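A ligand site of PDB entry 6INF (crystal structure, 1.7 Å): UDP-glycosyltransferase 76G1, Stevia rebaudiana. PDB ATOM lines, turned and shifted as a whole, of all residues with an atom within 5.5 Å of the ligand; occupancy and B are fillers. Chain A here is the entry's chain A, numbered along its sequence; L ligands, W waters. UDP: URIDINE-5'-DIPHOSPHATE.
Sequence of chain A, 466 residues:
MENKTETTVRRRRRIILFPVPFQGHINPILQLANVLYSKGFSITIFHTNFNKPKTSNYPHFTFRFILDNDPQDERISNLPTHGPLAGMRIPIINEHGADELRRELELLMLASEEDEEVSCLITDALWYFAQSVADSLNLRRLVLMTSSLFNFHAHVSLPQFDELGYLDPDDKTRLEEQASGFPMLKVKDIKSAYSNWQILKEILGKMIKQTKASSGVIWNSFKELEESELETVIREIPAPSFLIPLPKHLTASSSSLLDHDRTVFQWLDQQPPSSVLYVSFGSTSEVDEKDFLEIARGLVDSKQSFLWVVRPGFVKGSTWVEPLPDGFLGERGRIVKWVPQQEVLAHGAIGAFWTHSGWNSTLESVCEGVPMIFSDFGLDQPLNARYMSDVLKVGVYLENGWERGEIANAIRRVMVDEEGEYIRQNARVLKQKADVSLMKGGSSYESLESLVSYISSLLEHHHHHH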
ATOM      1  N   GLN A  23      26.060  -3.386 -13.125  1.00  0.00           N
ATOM      2  CA  GLN A  23      27.079  -3.072 -12.122  1.00  0.00           C
ATOM      3  C   GLN A  23      27.675  -4.307 -11.453  1.00  0.00           C
ATOM      4  O   GLN A  23      28.892  -4.390 -11.333  1.00  0.00           O
ATOM      5  CB  GLN A  23      26.561  -2.144 -11.042  1.00  0.00           C
ATOM      6  CG  GLN A  23      27.706  -1.557 -10.209  1.00  0.00           C
ATOM      7  CD  GLN A  23      28.474  -0.493 -10.956  1.00  0.00           C
ATOM      8  OE1 GLN A  23      27.994   0.616 -11.103  1.00  0.00           O
ATOM      9  NE2 GLN A  23      29.636  -0.833 -11.468  1.00  0.00           N
ATOM     10  N   GLY A  24      26.805  -5.241 -11.058  1.00  0.00           N
ATOM     11  CA  GLY A  24      27.215  -6.497 -10.396  1.00  0.00           C
ATOM     12  C   GLY A  24      27.967  -7.461 -11.266  1.00  0.00           C
ATOM     13  O   GLY A  24      28.469  -8.466 -10.779  1.00  0.00           O
ATOM     14  N   ASN A  27      31.704  -5.088 -12.418  1.00  0.00           N
ATOM     15  CA  ASN A  27      32.637  -5.011 -11.297  1.00  0.00           C
ATOM     16  C   ASN A  27      33.589  -6.178 -11.221  1.00  0.00           C
ATOM     17  O   ASN A  27      34.797  -5.979 -11.336  1.00  0.00           O
ATOM     18  CB  ASN A  27      31.909  -4.742  -9.997  1.00  0.00           C
ATOM     19  CG  ASN A  27      31.487  -3.297  -9.872  1.00  0.00           C
ATOM     20  OD1 ASN A  27      31.729  -2.492 -10.793  1.00  0.00           O
ATOM     21  ND2 ASN A  27      30.870  -2.938  -8.748  1.00  0.00           N
ATOM     22  N   ALA A 252      36.262  -2.369  -6.725  1.00  0.00           N
ATOM     23  CA  ALA A 252      35.643  -2.079  -8.029  1.00  0.00           C
ATOM     24  C   ALA A 252      35.343  -0.585  -8.262  1.00  0.00           C
ATOM     25  O   ALA A 252      34.521  -0.240  -9.138  1.00  0.00           O
ATOM     26  CB  ALA A 252      34.369  -2.898  -8.199  1.00  0.00           C
ATOM     27  N   SER A 256      32.734   1.825 -11.362  1.00  0.00           N
ATOM     28  CA  SER A 256      31.465   2.431 -10.999  1.00  0.00           C
ATOM     29  C   SER A 256      30.771   3.113 -12.178  1.00  0.00           C
ATOM     30  O   SER A 256      31.395   3.919 -12.869  1.00  0.00           O
ATOM     31  CB  SER A 256      31.663   3.501  -9.941  1.00  0.00           C
ATOM     32  OG  SER A 256      30.425   4.030  -9.543  1.00  0.00           O
ATOM     33  N   HIS A 260      30.045   8.637  -7.271  1.00  0.00           N
ATOM     34  CA  HIS A 260      30.171   8.407  -5.833  1.00  0.00           C
ATOM     35  C   HIS A 260      29.813   9.649  -5.047  1.00  0.00           C
ATOM     36  O   HIS A 260      30.265  10.751  -5.394  1.00  0.00           O
ATOM     37  CB  HIS A 260      31.605   8.030  -5.504  1.00  0.00           C
ATOM     38  CG  HIS A 260      31.996   6.694  -6.020  1.00  0.00           C
ATOM     39  ND1 HIS A 260      33.209   6.436  -6.617  1.00  0.00           N
ATOM     40  CD2 HIS A 260      31.302   5.527  -6.053  1.00  0.00           C
ATOM     41  CE1 HIS A 260      33.255   5.168  -6.977  1.00  0.00           C
ATOM     42  NE2 HIS A 260      32.113   4.596  -6.627  1.00  0.00           N
ATOM     43  N   TYR A 278      25.879   0.111   7.679  1.00  0.00           N
ATOM     44  CA  TYR A 278      25.761   0.405   6.251  1.00  0.00           C
ATOM     45  C   TYR A 278      24.585  -0.411   5.734  1.00  0.00           C
ATOM     46  O   TYR A 278      24.446  -1.575   6.059  1.00  0.00           O
ATOM     47  CB  TYR A 278      27.074   0.079   5.554  1.00  0.00           C
ATOM     48  CG  TYR A 278      27.027   0.213   4.053  1.00  0.00           C
ATOM     49  CD1 TYR A 278      26.782   1.433   3.466  1.00  0.00           C
ATOM     50  CD2 TYR A 278      27.126  -0.889   3.240  1.00  0.00           C
ATOM     51  CE1 TYR A 278      26.695   1.569   2.100  1.00  0.00           C
ATOM     52  CE2 TYR A 278      27.021  -0.791   1.863  1.00  0.00           C
ATOM     53  CZ  TYR A 278      26.815   0.470   1.308  1.00  0.00           C
ATOM     54  OH  TYR A 278      26.723   0.591  -0.043  1.00  0.00           O
ATOM     55  N   SER A 280      22.170  -1.323   2.259  1.00  0.00           N
ATOM     56  CA  SER A 280      21.949  -1.206   0.830  1.00  0.00           C
ATOM     57  C   SER A 280      21.196  -2.418   0.347  1.00  0.00           C
ATOM     58  O   SER A 280      21.651  -3.541   0.545  1.00  0.00           O
ATOM     59  CB  SER A 280      23.273  -1.043   0.094  1.00  0.00           C
ATOM     60  OG  SER A 280      23.063  -0.981  -1.316  1.00  0.00           O
ATOM     61  N   GLY A 282      20.194  -3.163  -2.849  1.00  0.00           N
ATOM     62  CA  GLY A 282      20.497  -3.691  -4.146  1.00  0.00           C
ATOM     63  C   GLY A 282      19.984  -2.865  -5.285  1.00  0.00           C
ATOM     64  O   GLY A 282      19.112  -1.997  -5.111  1.00  0.00           O
ATOM     65  N   SER A 283      20.524  -3.167  -6.457  1.00  0.00           N
ATOM     66  CA  SER A 283      20.351  -2.334  -7.652  1.00  0.00           C
ATOM     67  C   SER A 283      18.932  -2.309  -8.173  1.00  0.00           C
ATOM     68  O   SER A 283      18.470  -1.265  -8.655  1.00  0.00           O
ATOM     69  CB  SER A 283      21.269  -2.804  -8.780  1.00  0.00           C
ATOM     70  OG  SER A 283      22.635  -2.701  -8.390  1.00  0.00           O
ATOM     71  N   THR A 284      18.254  -3.457  -8.143  1.00  0.00           N
ATOM     72  CA  THR A 284      16.950  -3.593  -8.764  1.00  0.00           C
ATOM     73  C   THR A 284      15.848  -4.039  -7.799  1.00  0.00           C
ATOM     74  O   THR A 284      14.676  -4.197  -8.205  1.00  0.00           O
ATOM     75  CB  THR A 284      17.055  -4.571  -9.956  1.00  0.00           C
ATOM     76  OG1 THR A 284      17.530  -5.839  -9.484  1.00  0.00           O
ATOM     77  CG2 THR A 284      18.038  -4.048 -10.991  1.00  0.00           C
ATOM     78  N   VAL A 309      22.153   3.448   1.428  1.00  0.00           N
ATOM     79  CA  VAL A 309      22.115   3.728   0.001  1.00  0.00           C
ATOM     80  C   VAL A 309      20.726   3.267  -0.467  1.00  0.00           C
ATOM     81  O   VAL A 309      20.423   2.097  -0.369  1.00  0.00           O
ATOM     82  CB  VAL A 309      23.189   2.937  -0.774  1.00  0.00           C
ATOM     83  CG1 VAL A 309      22.982   3.067  -2.290  1.00  0.00           C
ATOM     84  CG2 VAL A 309      24.572   3.435  -0.394  1.00  0.00           C
ATOM     85  N   LYS A 337      22.530   8.138  -2.502  1.00  0.00           N
ATOM     86  CA  LYS A 337      22.203   7.334  -3.674  1.00  0.00           C
ATOM     87  C   LYS A 337      23.239   6.305  -4.098  1.00  0.00           C
ATOM     88  O   LYS A 337      22.869   5.316  -4.731  1.00  0.00           O
ATOM     89  CB  LYS A 337      21.926   8.241  -4.868  1.00  0.00           C
ATOM     90  CG  LYS A 337      20.700   9.112  -4.625  1.00  0.00           C
ATOM     91  CD  LYS A 337      20.184   9.720  -5.896  1.00  0.00           C
ATOM     92  CE  LYS A 337      18.848  10.405  -5.646  1.00  0.00           C
ATOM     93  NZ  LYS A 337      18.624  11.436  -6.680  1.00  0.00           N
ATOM     94  N   TRP A 338      24.515   6.548  -3.804  1.00  0.00           N
ATOM     95  CA  TRP A 338      25.619   5.750  -4.345  1.00  0.00           C
ATOM     96  C   TRP A 338      26.933   6.087  -3.647  1.00  0.00           C
ATOM     97  O   TRP A 338      27.273   7.260  -3.504  1.00  0.00           O
ATOM     98  CB  TRP A 338      25.799   6.020  -5.826  1.00  0.00           C
ATOM     99  CG  TRP A 338      26.634   5.021  -6.501  1.00  0.00           C
ATOM    100  CD1 TRP A 338      27.873   5.201  -6.983  1.00  0.00           C
ATOM    101  CD2 TRP A 338      26.292   3.655  -6.743  1.00  0.00           C
ATOM    102  NE1 TRP A 338      28.348   4.033  -7.527  1.00  0.00           N
ATOM    103  CE2 TRP A 338      27.385   3.071  -7.399  1.00  0.00           C
ATOM    104  CE3 TRP A 338      25.164   2.875  -6.482  1.00  0.00           C
ATOM    105  CZ2 TRP A 338      27.382   1.733  -7.811  1.00  0.00           C
ATOM    106  CZ3 TRP A 338      25.149   1.540  -6.901  1.00  0.00           C
ATOM    107  CH2 TRP A 338      26.262   0.987  -7.553  1.00  0.00           C
ATOM    108  N   VAL A 339      27.670   5.051  -3.263  1.00  0.00           N
ATOM    109  CA  VAL A 339      28.961   5.224  -2.595  1.00  0.00           C
ATOM    110  C   VAL A 339      29.994   4.300  -3.211  1.00  0.00           C
ATOM    111  O   VAL A 339      29.630   3.423  -3.995  1.00  0.00           O
ATOM    112  CB  VAL A 339      28.853   4.939  -1.084  1.00  0.00           C
ATOM    113  CG1 VAL A 339      27.814   5.824  -0.458  1.00  0.00           C
ATOM    114  CG2 VAL A 339      28.570   3.455  -0.819  1.00  0.00           C
ATOM    115  N   PRO A 340      31.291   4.493  -2.885  1.00  0.00           N
ATOM    116  CA  PRO A 340      32.243   3.437  -3.236  1.00  0.00           C
ATOM    117  C   PRO A 340      32.103   2.380  -2.153  1.00  0.00           C
ATOM    118  O   PRO A 340      32.685   2.498  -1.081  1.00  0.00           O
ATOM    119  CB  PRO A 340      33.596   4.151  -3.242  1.00  0.00           C
ATOM    120  CG  PRO A 340      33.365   5.494  -2.654  1.00  0.00           C
ATOM    121  CD  PRO A 340      31.954   5.617  -2.204  1.00  0.00           C
ATOM    122  N   GLN A 341      31.345   1.334  -2.451  1.00  0.00           N
ATOM    123  CA  GLN A 341      30.827   0.500  -1.409  1.00  0.00           C
ATOM    124  C   GLN A 341      31.931  -0.216  -0.644  1.00  0.00           C
ATOM    125  O   GLN A 341      31.913  -0.200   0.575  1.00  0.00           O
ATOM    126  CB  GLN A 341      29.758  -0.479  -1.905  1.00  0.00           C
ATOM    127  CG  GLN A 341      29.363  -1.517  -0.868  1.00  0.00           C
ATOM    128  CD  GLN A 341      28.129  -2.317  -1.273  1.00  0.00           C
ATOM    129  OE1 GLN A 341      27.029  -1.785  -1.315  1.00  0.00           O
ATOM    130  NE2 GLN A 341      28.320  -3.594  -1.597  1.00  0.00           N
ATOM    131  N   GLN A 342      32.874  -0.832  -1.341  1.00  0.00           N
ATOM    132  CA  GLN A 342      33.908  -1.564  -0.632  1.00  0.00           C
ATOM    133  C   GLN A 342      34.792  -0.636   0.229  1.00  0.00           C
ATOM    134  O   GLN A 342      35.108  -0.959   1.384  1.00  0.00           O
ATOM    135  CB  GLN A 342      34.753  -2.383  -1.576  1.00  0.00           C
ATOM    136  CG  GLN A 342      35.576  -3.367  -0.784  1.00  0.00           C
ATOM    137  CD  GLN A 342      36.385  -4.285  -1.650  1.00  0.00           C
ATOM    138  OE1 GLN A 342      36.120  -4.424  -2.833  1.00  0.00           O
ATOM    139  NE2 GLN A 342      37.436  -4.876  -1.073  1.00  0.00           N
ATOM    140  N   HIS A 356      21.021  -6.914   0.801  1.00  0.00           N
ATOM    141  CA  HIS A 356      20.115  -7.800   0.099  1.00  0.00           C
ATOM    142  C   HIS A 356      20.716  -9.141  -0.281  1.00  0.00           C
ATOM    143  O   HIS A 356      20.002  -9.961  -0.823  1.00  0.00           O
ATOM    144  CB  HIS A 356      19.580  -7.144  -1.154  1.00  0.00           C
ATOM    145  CG  HIS A 356      20.560  -7.057  -2.283  1.00  0.00           C
ATOM    146  ND1 HIS A 356      21.851  -6.562  -2.152  1.00  0.00           N
ATOM    147  CD2 HIS A 356      20.406  -7.353  -3.587  1.00  0.00           C
ATOM    148  CE1 HIS A 356      22.436  -6.566  -3.340  1.00  0.00           C
ATOM    149  NE2 HIS A 356      21.577  -7.037  -4.230  1.00  0.00           N
ATOM    150  N   GLY A 358      23.157  -9.781  -2.422  1.00  0.00           N
ATOM    151  CA  GLY A 358      23.800  -9.915  -3.705  1.00  0.00           C
ATOM    152  C   GLY A 358      25.215 -10.417  -3.508  1.00  0.00           C
ATOM    153  O   GLY A 358      25.860 -10.134  -2.484  1.00  0.00           O
ATOM    154  N   TRP A 359      25.685 -11.186  -4.459  1.00  0.00           N
ATOM    155  CA  TRP A 359      26.972 -11.826  -4.209  1.00  0.00           C
ATOM    156  C   TRP A 359      28.175 -10.857  -4.109  1.00  0.00           C
ATOM    157  O   TRP A 359      29.039 -11.034  -3.245  1.00  0.00           O
ATOM    158  CB  TRP A 359      27.257 -12.896  -5.258  1.00  0.00           C
ATOM    159  CG  TRP A 359      28.462 -13.707  -4.931  1.00  0.00           C
ATOM    160  CD1 TRP A 359      29.618 -13.767  -5.629  1.00  0.00           C
ATOM    161  CD2 TRP A 359      28.674 -14.503  -3.761  1.00  0.00           C
ATOM    162  NE1 TRP A 359      30.517 -14.544  -5.016  1.00  0.00           N
ATOM    163  CE2 TRP A 359      29.969 -15.048  -3.873  1.00  0.00           C
ATOM    164  CE3 TRP A 359      27.890 -14.845  -2.674  1.00  0.00           C
ATOM    165  CZ2 TRP A 359      30.505 -15.919  -2.936  1.00  0.00           C
ATOM    166  CZ3 TRP A 359      28.417 -15.665  -1.720  1.00  0.00           C
ATOM    167  CH2 TRP A 359      29.728 -16.197  -1.854  1.00  0.00           C
ATOM    168  N   ASN A 360      28.272  -9.869  -4.981  1.00  0.00           N
ATOM    169  CA  ASN A 360      29.399  -8.926  -4.822  1.00  0.00           C
ATOM    170  C   ASN A 360      29.411  -8.264  -3.484  1.00  0.00           C
ATOM    171  O   ASN A 360      30.466  -8.147  -2.834  1.00  0.00           O
ATOM    172  CB  ASN A 360      29.442  -7.838  -5.886  1.00  0.00           C
ATOM    173  CG  ASN A 360      29.661  -8.404  -7.252  1.00  0.00           C
ATOM    174  OD1 ASN A 360      30.773  -8.824  -7.574  1.00  0.00           O
ATOM    175  ND2 ASN A 360      28.602  -8.466  -8.055  1.00  0.00           N
ATOM    176  N   SER A 361      28.232  -7.831  -3.050  1.00  0.00           N
ATOM    177  CA  SER A 361      28.090  -7.165  -1.762  1.00  0.00           C
ATOM    178  C   SER A 361      28.470  -8.067  -0.639  1.00  0.00           C
ATOM    179  O   SER A 361      29.182  -7.659   0.276  1.00  0.00           O
ATOM    180  CB  SER A 361      26.663  -6.689  -1.567  1.00  0.00           C
ATOM    181  OG  SER A 361      26.365  -5.626  -2.433  1.00  0.00           O
ATOM    182  N   THR A 362      27.967  -9.281  -0.681  1.00  0.00           N
ATOM    183  CA  THR A 362      28.254 -10.282   0.329  1.00  0.00           C
ATOM    184  C   THR A 362      29.767 -10.519   0.414  1.00  0.00           C
ATOM    185  O   THR A 362      30.391 -10.454   1.483  1.00  0.00           O
ATOM    186  CB  THR A 362      27.471 -11.564   0.064  1.00  0.00           C
ATOM    187  OG1 THR A 362      26.063 -11.285   0.084  1.00  0.00           O
ATOM    188  CG2 THR A 362      27.753 -12.546   1.144  1.00  0.00           C
ATOM    189  N   GLU A 364      32.271  -8.594  -0.759  1.00  0.00           N
ATOM    190  CA  GLU A 364      32.963  -7.396  -0.332  1.00  0.00           C
ATOM    191  C   GLU A 364      32.945  -7.282   1.162  1.00  0.00           C
ATOM    192  O   GLU A 364      33.952  -6.987   1.798  1.00  0.00           O
ATOM    193  CB  GLU A 364      32.321  -6.152  -0.952  1.00  0.00           C
ATOM    194  CG  GLU A 364      32.653  -5.997  -2.431  1.00  0.00           C
ATOM    195  CD  GLU A 364      31.596  -5.210  -3.194  1.00  0.00           C
ATOM    196  OE1 GLU A 364      30.812  -4.455  -2.585  1.00  0.00           O
ATOM    197  OE2 GLU A 364      31.580  -5.302  -4.436  1.00  0.00           O
ATOM    198  N   GLN A 381      19.862 -14.606  -3.861  1.00  0.00           N
ATOM    199  CA  GLN A 381      19.954 -13.880  -2.592  1.00  0.00           C
ATOM    200  C   GLN A 381      19.572 -14.690  -1.338  1.00  0.00           C
ATOM    201  O   GLN A 381      20.310 -14.648  -0.365  1.00  0.00           O
ATOM    202  CB  GLN A 381      19.186 -12.580  -2.663  1.00  0.00           C
ATOM    203  CG  GLN A 381      19.850 -11.619  -3.615  1.00  0.00           C
ATOM    204  CD  GLN A 381      18.916 -10.583  -4.156  1.00  0.00           C
ATOM    205  OE1 GLN A 381      17.983 -10.187  -3.491  1.00  0.00           O
ATOM    206  NE2 GLN A 381      19.219 -10.087  -5.329  1.00  0.00           N
HETATM  207  N1  UDP L   1      27.810  -0.786  -5.163  1.00  0.00           N
HETATM  208  C2  UDP L   1      28.549   0.408  -5.019  1.00  0.00           C
HETATM  209  N3  UDP L   1      27.970   1.434  -4.408  1.00  0.00           N
HETATM  210  C4  UDP L   1      26.724   1.409  -3.945  1.00  0.00           C
HETATM  211  C5  UDP L   1      25.967   0.235  -4.041  1.00  0.00           C
HETATM  212  C6  UDP L   1      26.558  -0.850  -4.690  1.00  0.00           C
HETATM  213  O2  UDP L   1      29.713   0.480  -5.443  1.00  0.00           O
HETATM  214  O4  UDP L   1      26.238   2.414  -3.382  1.00  0.00           O
HETATM  215  C1' UDP L   1      28.430  -1.920  -5.807  1.00  0.00           C
HETATM  216  C2' UDP L   1      28.759  -3.027  -4.802  1.00  0.00           C
HETATM  217  O2' UDP L   1      30.022  -2.786  -4.190  1.00  0.00           O
HETATM  218  C3' UDP L   1      28.786  -4.227  -5.722  1.00  0.00           C
HETATM  219  C4' UDP L   1      27.731  -3.905  -6.789  1.00  0.00           C
HETATM  220  O4' UDP L   1      27.528  -2.503  -6.745  1.00  0.00           O
HETATM  221  O3' UDP L   1      30.046  -4.411  -6.303  1.00  0.00           O
HETATM  222  C5' UDP L   1      26.394  -4.558  -6.490  1.00  0.00           C
HETATM  223  O5' UDP L   1      26.525  -5.951  -6.726  1.00  0.00           O
HETATM  224  PA  UDP L   1      25.651  -7.048  -5.971  1.00  0.00           P
HETATM  225  O1A UDP L   1      26.093  -8.351  -6.518  1.00  0.00           O
HETATM  226  O2A UDP L   1      25.798  -6.862  -4.488  1.00  0.00           O
HETATM  227  O3A UDP L   1      24.077  -6.852  -6.159  1.00  0.00           O
HETATM  228  PB  UDP L   1      23.099  -6.149  -7.228  1.00  0.00           P
HETATM  229  O1B UDP L   1      21.824  -6.908  -6.927  1.00  0.00           O
HETATM  230  O2B UDP L   1      23.717  -6.359  -8.576  1.00  0.00           O
HETATM  231  O3B UDP L   1      22.995  -4.727  -6.752  1.00  0.00           O
HETATM  232  O   HOH W   1      31.710   1.869  -6.541  1.00  0.00           O
HETATM  233  O   HOH W   2      24.075  -8.307 -10.080  1.00  0.00           O
HETATM  234  O   HOH W   3      24.013  -4.728 -10.746  1.00  0.00           O
HETATM  235  O   HOH W   4      19.347  -6.047  -7.513  1.00  0.00           O
HETATM  236  O   HOH W   5      23.915  -2.971  -4.786  1.00  0.00           O
HETATM  237  O   HOH W   6      32.564  -1.649  -4.180  1.00  0.00           O
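The side-chain carboxylate of Glu 364 sits at hydrogen-bond distance from an oxygen (O2') of the ligand (2.4 Å). An oxygen (O2A) of the ligand lies within hydrogen-bond range of the backbone NH of Ser 361 (3.0 Å). The side-chain hydroxyl of Ser 361 is in hydrogen-bond range of an oxygen (O2A) of the ligand, at 2.5 Å. The backbone NH of Val 339 sits at hydrogen-bond distance from an oxygen (O4) of the ligand. The backbone carbonyl oxygen (O) of Val 339 is in hydrogen-bond range of a nitrogen (N3) of the ligand (2.6 Å). N of Ser 283 is in hydrogen-bond range of O3B of the ligand (2.9 Å). An oxygen (O3B) of the ligand lies within hydrogen-bond range of the side-chain hydroxyl (OG) of Ser 283 (2.6 Å). O1B of the ligand sits at hydrogen-bond distance from NE2 of His 356, 2.7 Å away. The backbone NH of Asn 360 lies within hydrogen-bond range of an oxygen (O1A) of the ligand, at 3.1 Å. O1A of the ligand sits at hydrogen-bond distance from ND2 of Asn 360, at 2.9 Å. An oxygen (O3') of the ligand lies within hydrogen-bond range of the side-chain amide nitrogen (ND2) of Asn 27 (3.0 Å). The side-chain amide nitrogen of Gln 341 is in hydrogen-bond range of an oxygen (O2') of the ligand, at 3.2 Å.
OE1 of Glu 364 is in hydrogen-bond range of NE2 of Gln 341 (2.8 Å). OG of Ser 361 is in hydrogen-bond range of NE2 of Gln 341, at 2.9 Å. The backbone NH of His 356 sits at hydrogen-bond distance from the backbone carbonyl oxygen of Ser 280. O of His 356 sits close to OE1 of Gln 381 (3.4 Å). The side-chain amide nitrogen (NE2) of Gln 23 lies within hydrogen-bond range of the side-chain amide oxygen (OD1) of Asn 27 (2.8 Å). The side-chain amide oxygen (OE1) of Gln 341 lies within hydrogen-bond range of the side-chain hydroxyl (OH) of Tyr 278 (2.7 Å). The side-chain hydroxyl (OG) of Ser 256 lies within hydrogen-bond range of the indole nitrogen (NE1) of Trp 338, at 2.9 Å. The backbone carbonyl oxygen of Gly 358 is in hydrogen-bond range of the side-chain hydroxyl of Thr 362.
Merely in contact with the ligand: Gln 23, Gly 24, Tyr 278, Gly 282, Val 309, Trp 338, Gly 358 and Trp 359. Hydrophobic or aromatic side chains that line the ligand: Val 309, Trp 338, Val 339 and His 356. Along chain A the residues within 4 Å of the ligand span positions 23 to 364.
Water W1 lies within hydrogen-bond range of an oxygen (O2) of the ligand (2.7 Å) and a ring nitrogen (NE2) of His 260 (2.8 Å). Water W4 lies within hydrogen-bond range of an oxygen (O1B) of the ligand (2.7 Å), the side-chain hydroxyl of Thr 284 (2.7 Å) and the backbone NH of Ser 283 (3.3 Å). Water W3 lies within hydrogen-bond range of an oxygen (O2B) of the ligand, the backbone NH of Gly 24, the side-chain hydroxyl of Ser 283 and the backbone NH of Gln 23. Water W6 bridges O2' of the ligand (2.8 Å) and N of Gln 342 (3.0 Å).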
